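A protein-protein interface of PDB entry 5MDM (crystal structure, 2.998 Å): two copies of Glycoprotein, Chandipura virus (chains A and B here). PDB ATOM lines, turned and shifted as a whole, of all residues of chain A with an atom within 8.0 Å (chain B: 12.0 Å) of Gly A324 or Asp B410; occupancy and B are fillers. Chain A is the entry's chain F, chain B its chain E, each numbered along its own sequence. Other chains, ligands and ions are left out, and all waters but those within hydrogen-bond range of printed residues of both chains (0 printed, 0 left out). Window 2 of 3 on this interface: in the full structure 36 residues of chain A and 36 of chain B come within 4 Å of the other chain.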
ATOM      1  N   VAL A  17       5.461  27.273 -19.001  1.00  0.00           N
ATOM      2  CA  VAL A  17       6.831  26.975 -19.385  1.00  0.00           C
ATOM      3  C   VAL A  17       6.964  25.488 -19.724  1.00  0.00           C
ATOM      4  O   VAL A  17       6.943  24.629 -18.841  1.00  0.00           O
ATOM      5  CB  VAL A  17       7.856  27.412 -18.301  1.00  0.00           C
ATOM      6  CG1 VAL A  17       7.360  27.088 -16.899  1.00  0.00           C
ATOM      7  CG2 VAL A  17       9.217  26.784 -18.559  1.00  0.00           C
ATOM      8  N   THR A  18       7.049  25.193 -21.017  1.00  0.00           N
ATOM      9  CA  THR A  18       7.367  23.846 -21.488  1.00  0.00           C
ATOM     10  C   THR A  18       8.672  23.985 -22.261  1.00  0.00           C
ATOM     11  O   THR A  18       9.333  23.003 -22.607  1.00  0.00           O
ATOM     12  CB  THR A  18       6.244  23.258 -22.393  1.00  0.00           C
ATOM     13  OG1 THR A  18       4.978  23.372 -21.732  1.00  0.00           O
ATOM     14  CG2 THR A  18       6.501  21.784 -22.709  1.00  0.00           C
ATOM     15  N   VAL A 294      12.376  19.450 -12.326  1.00  0.00           N
ATOM     16  CA  VAL A 294      11.465  19.699 -13.440  1.00  0.00           C
ATOM     17  C   VAL A 294      11.786  18.806 -14.635  1.00  0.00           C
ATOM     18  O   VAL A 294      10.898  18.143 -15.177  1.00  0.00           O
ATOM     19  CB  VAL A 294      11.476  21.182 -13.864  1.00  0.00           C
ATOM     20  CG1 VAL A 294      10.789  21.363 -15.197  1.00  0.00           C
ATOM     21  CG2 VAL A 294      10.807  22.039 -12.803  1.00  0.00           C
ATOM     22  N   LYS A 297      10.976  15.307 -14.337  1.00  0.00           N
ATOM     23  CA  LYS A 297       9.530  15.172 -14.177  1.00  0.00           C
ATOM     24  C   LYS A 297       9.145  14.651 -12.795  1.00  0.00           C
ATOM     25  O   LYS A 297       8.173  13.914 -12.649  1.00  0.00           O
ATOM     26  CB  LYS A 297       8.935  14.293 -15.279  1.00  0.00           C
ATOM     27  CG  LYS A 297       9.213  14.805 -16.682  1.00  0.00           C
ATOM     28  CD  LYS A 297       8.563  13.932 -17.739  1.00  0.00           C
ATOM     29  CE  LYS A 297       8.877  14.439 -19.140  1.00  0.00           C
ATOM     30  NZ  LYS A 297       8.451  15.855 -19.328  1.00  0.00           N
ATOM     31  N   THR A 320       4.625  29.863 -10.703  1.00  0.00           N
ATOM     32  CA  THR A 320       3.478  29.332  -9.983  1.00  0.00           C
ATOM     33  C   THR A 320       2.973  28.110 -10.731  1.00  0.00           C
ATOM     34  O   THR A 320       3.517  27.755 -11.773  1.00  0.00           O
ATOM     35  CB  THR A 320       2.351  30.376  -9.853  1.00  0.00           C
ATOM     36  OG1 THR A 320       1.468  29.998  -8.792  1.00  0.00           O
ATOM     37  CG2 THR A 320       1.573  30.501 -11.153  1.00  0.00           C
ATOM     38  N   VAL A 321       1.951  27.451 -10.201  1.00  0.00           N
ATOM     39  CA  VAL A 321       1.370  26.309 -10.893  1.00  0.00           C
ATOM     40  C   VAL A 321      -0.115  26.538 -11.152  1.00  0.00           C
ATOM     41  O   VAL A 321      -0.909  26.655 -10.218  1.00  0.00           O
ATOM     42  CB  VAL A 321       1.572  24.996 -10.112  1.00  0.00           C
ATOM     43  CG1 VAL A 321       1.183  23.814 -10.976  1.00  0.00           C
ATOM     44  CG2 VAL A 321       3.018  24.862  -9.659  1.00  0.00           C
ATOM     45  N   ILE A 322      -0.478  26.607 -12.430  1.00  0.00           N
ATOM     46  CA  ILE A 322      -1.856  26.875 -12.840  1.00  0.00           C
ATOM     47  C   ILE A 322      -2.448  25.668 -13.549  1.00  0.00           C
ATOM     48  O   ILE A 322      -1.985  25.290 -14.626  1.00  0.00           O
ATOM     49  CB  ILE A 322      -1.936  28.076 -13.798  1.00  0.00           C
ATOM     50  CG1 ILE A 322      -1.246  29.294 -13.192  1.00  0.00           C
ATOM     51  CG2 ILE A 322      -3.374  28.406 -14.111  1.00  0.00           C
ATOM     52  CD1 ILE A 322      -1.021  30.396 -14.182  1.00  0.00           C
ATOM     53  N   ASN A 323      -3.475  25.080 -12.942  1.00  0.00           N
ATOM     54  CA  ASN A 323      -4.099  23.869 -13.465  1.00  0.00           C
ATOM     55  C   ASN A 323      -3.072  22.776 -13.736  1.00  0.00           C
ATOM     56  O   ASN A 323      -3.166  22.048 -14.725  1.00  0.00           O
ATOM     57  CB  ASN A 323      -4.915  24.174 -14.725  1.00  0.00           C
ATOM     58  CG  ASN A 323      -6.277  24.766 -14.410  1.00  0.00           C
ATOM     59  OD1 ASN A 323      -7.070  24.168 -13.681  1.00  0.00           O
ATOM     60  ND2 ASN A 323      -6.551  25.954 -14.950  1.00  0.00           N
ATOM     61  N   GLY A 324      -2.083  22.675 -12.856  1.00  0.00           N
ATOM     62  CA  GLY A 324      -1.066  21.647 -12.975  1.00  0.00           C
ATOM     63  C   GLY A 324       0.067  22.011 -13.914  1.00  0.00           C
ATOM     64  O   GLY A 324       1.052  21.281 -14.021  1.00  0.00           O
ATOM     65  N   THR A 325      -0.065  23.141 -14.596  1.00  0.00           N
ATOM     66  CA  THR A 325       0.971  23.594 -15.512  1.00  0.00           C
ATOM     67  C   THR A 325       1.932  24.555 -14.828  1.00  0.00           C
ATOM     68  O   THR A 325       1.511  25.559 -14.256  1.00  0.00           O
ATOM     69  CB  THR A 325       0.365  24.304 -16.725  1.00  0.00           C
ATOM     70  OG1 THR A 325      -0.401  23.368 -17.493  1.00  0.00           O
ATOM     71  CG2 THR A 325       1.463  24.905 -17.594  1.00  0.00           C
ATOM     72  N   LEU A 326       3.223  24.243 -14.882  1.00  0.00           N
ATOM     73  CA  LEU A 326       4.236  25.157 -14.372  1.00  0.00           C
ATOM     74  C   LEU A 326       4.220  26.413 -15.227  1.00  0.00           C
ATOM     75  O   LEU A 326       4.352  26.351 -16.447  1.00  0.00           O
ATOM     76  CB  LEU A 326       5.621  24.512 -14.389  1.00  0.00           C
ATOM     77  CG  LEU A 326       6.741  25.334 -13.759  1.00  0.00           C
ATOM     78  CD1 LEU A 326       6.343  25.754 -12.359  1.00  0.00           C
ATOM     79  CD2 LEU A 326       8.040  24.547 -13.733  1.00  0.00           C
ATOM     80  N   SER A 327       4.035  27.552 -14.578  1.00  0.00           N
ATOM     81  CA  SER A 327       3.844  28.807 -15.280  1.00  0.00           C
ATOM     82  C   SER A 327       4.777  29.860 -14.719  1.00  0.00           C
ATOM     83  O   SER A 327       5.173  29.795 -13.552  1.00  0.00           O
ATOM     84  CB  SER A 327       2.396  29.276 -15.138  1.00  0.00           C
ATOM     85  OG  SER A 327       1.495  28.226 -15.437  1.00  0.00           O
ATOM     86  N   PHE A 365      -4.307  30.645  -7.420  1.00  0.00           N
ATOM     87  CA  PHE A 365      -4.691  29.552  -8.301  1.00  0.00           C
ATOM     88  C   PHE A 365      -4.995  28.333  -7.453  1.00  0.00           C
ATOM     89  O   PHE A 365      -4.379  28.146  -6.413  1.00  0.00           O
ATOM     90  CB  PHE A 365      -3.577  29.262  -9.304  1.00  0.00           C
ATOM     91  CG  PHE A 365      -3.223  30.443 -10.159  1.00  0.00           C
ATOM     92  CD1 PHE A 365      -3.910  30.694 -11.334  1.00  0.00           C
ATOM     93  CD2 PHE A 365      -2.216  31.313  -9.778  1.00  0.00           C
ATOM     94  CE1 PHE A 365      -3.591  31.783 -12.115  1.00  0.00           C
ATOM     95  CE2 PHE A 365      -1.892  32.406 -10.556  1.00  0.00           C
ATOM     96  CZ  PHE A 365      -2.580  32.642 -11.725  1.00  0.00           C
ATOM     97  N   LYS A 366      -5.959  27.521  -7.872  1.00  0.00           N
ATOM     98  CA  LYS A 366      -6.284  26.329  -7.099  1.00  0.00           C
ATOM     99  C   LYS A 366      -5.082  25.400  -7.066  1.00  0.00           C
ATOM    100  O   LYS A 366      -4.550  25.020  -8.105  1.00  0.00           O
ATOM    101  CB  LYS A 366      -7.509  25.599  -7.655  1.00  0.00           C
ATOM    102  CG  LYS A 366      -7.855  24.343  -6.866  1.00  0.00           C
ATOM    103  CD  LYS A 366      -9.231  23.812  -7.211  1.00  0.00           C
ATOM    104  CE  LYS A 366      -9.576  22.593  -6.368  1.00  0.00           C
ATOM    105  NZ  LYS A 366      -8.647  21.454  -6.623  1.00  0.00           N
ATOM    106  N   TYR A 367      -4.643  25.066  -5.859  1.00  0.00           N
ATOM    107  CA  TYR A 367      -3.510  24.174  -5.673  1.00  0.00           C
ATOM    108  C   TYR A 367      -3.928  23.058  -4.724  1.00  0.00           C
ATOM    109  O   TYR A 367      -3.614  23.087  -3.534  1.00  0.00           O
ATOM    110  CB  TYR A 367      -2.313  24.947  -5.119  1.00  0.00           C
ATOM    111  CG  TYR A 367      -1.009  24.180  -5.120  1.00  0.00           C
ATOM    112  CD1 TYR A 367      -0.316  23.947  -6.299  1.00  0.00           C
ATOM    113  CD2 TYR A 367      -0.461  23.706  -3.936  1.00  0.00           C
ATOM    114  CE1 TYR A 367       0.883  23.247  -6.296  1.00  0.00           C
ATOM    115  CE2 TYR A 367       0.733  23.008  -3.922  1.00  0.00           C
ATOM    116  CZ  TYR A 367       1.401  22.779  -5.102  1.00  0.00           C
ATOM    117  OH  TYR A 367       2.590  22.084  -5.085  1.00  0.00           O
ATOM    118  N   ALA B 406       5.568  17.551  -1.813  1.00  0.00           N
ATOM    119  CA  ALA B 406       5.735  17.602  -3.261  1.00  0.00           C
ATOM    120  C   ALA B 406       4.505  17.095  -3.999  1.00  0.00           C
ATOM    121  O   ALA B 406       3.864  16.136  -3.574  1.00  0.00           O
ATOM    122  CB  ALA B 406       6.964  16.807  -3.673  1.00  0.00           C
ATOM    123  N   ASN B 407       4.188  17.744  -5.113  1.00  0.00           N
ATOM    124  CA  ASN B 407       3.056  17.354  -5.942  1.00  0.00           C
ATOM    125  C   ASN B 407       3.445  17.354  -7.415  1.00  0.00           C
ATOM    126  O   ASN B 407       4.080  18.297  -7.886  1.00  0.00           O
ATOM    127  CB  ASN B 407       1.883  18.307  -5.719  1.00  0.00           C
ATOM    128  CG  ASN B 407       1.434  18.348  -4.273  1.00  0.00           C
ATOM    129  OD1 ASN B 407       1.324  17.313  -3.616  1.00  0.00           O
ATOM    130  ND2 ASN B 407       1.180  19.550  -3.766  1.00  0.00           N
ATOM    131  N   PRO B 408       3.062  16.297  -8.148  1.00  0.00           N
ATOM    132  CA  PRO B 408       3.399  16.141  -9.569  1.00  0.00           C
ATOM    133  C   PRO B 408       2.794  17.243 -10.442  1.00  0.00           C
ATOM    134  O   PRO B 408       1.867  17.934 -10.022  1.00  0.00           O
ATOM    135  CB  PRO B 408       2.783  14.785  -9.923  1.00  0.00           C
ATOM    136  CG  PRO B 408       1.688  14.600  -8.933  1.00  0.00           C
ATOM    137  CD  PRO B 408       2.205  15.202  -7.665  1.00  0.00           C
ATOM    138  N   LEU B 409       3.322  17.403 -11.649  1.00  0.00           N
ATOM    139  CA  LEU B 409       2.843  18.446 -12.548  1.00  0.00           C
ATOM    140  C   LEU B 409       2.115  17.880 -13.767  1.00  0.00           C
ATOM    141  O   LEU B 409       2.097  16.669 -13.977  1.00  0.00           O
ATOM    142  CB  LEU B 409       3.999  19.342 -12.991  1.00  0.00           C
ATOM    143  CG  LEU B 409       4.697  20.083 -11.857  1.00  0.00           C
ATOM    144  CD1 LEU B 409       5.687  21.090 -12.411  1.00  0.00           C
ATOM    145  CD2 LEU B 409       3.672  20.760 -10.964  1.00  0.00           C
ATOM    146  N   ASP B 410       1.523  18.777 -14.555  1.00  0.00           N
ATOM    147  CA  ASP B 410       0.783  18.431 -15.773  1.00  0.00           C
ATOM    148  C   ASP B 410      -0.329  17.410 -15.517  1.00  0.00           C
ATOM    149  O   ASP B 410      -1.511  17.704 -15.698  1.00  0.00           O
ATOM    150  CB  ASP B 410       1.729  17.930 -16.873  1.00  0.00           C
ATOM    151  CG  ASP B 410       2.998  18.763 -16.986  1.00  0.00           C
ATOM    152  OD1 ASP B 410       2.922  19.997 -16.801  1.00  0.00           O
ATOM    153  OD2 ASP B 410       4.073  18.183 -17.259  1.00  0.00           O
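The side-chain amide nitrogen of Asn B407 lies within hydrogen-bond range of the side-chain hydroxyl of Tyr A367, at 3.2 Å. N of Asp B410 sits at hydrogen-bond distance from O of Gly A324 (2.6 Å).
The backbone carbonyl oxygen (O) of Leu A326 lies within hydrogen-bond range of the backbone NH (N) of Val A17 (2.9 Å).
Among the printed residues, pairs that only touch across the chains: Val A321 with Leu B409, Gly A324 with Leu B409 and Leu A326 with Leu B409.
Of chain B, only Leu B409 (3.9 Å) comes within 4 Å of Val A321. No residue of chain B comes within 4 Å of Ile A322. No residue of chain B comes within 4 Å of Asn A323. Gly A324 touches two residues of chain B. Printed residues of chain B within 4 Å of Tyr A367: Asn B407 (3.2 Å). Of the printed residues of chain A, Asn B407 touches Tyr A367. Of the printed residues of chain A, Leu B409 touches Val A321 (3.9 Å), Gly A324 (3.6 Å) and Leu A326 (3.95 Å). Asp B410 touches just one residue of chain A: Gly A324 (2.6 Å). The nearest residue of chain B that does not touch Gly A324 is Pro B408 (5.3 Å). The nearest residue of chain A that does not touch Asp B410 is Thr A325 (4.3 Å).
Along chain A the printed residues that touch a printed residue of chain B span positions 321 to 367.
No position is printed for both chains. Of the 5 pairs that touch across the chains among the printed residues, none has its exchanged pair printed and touching as well.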
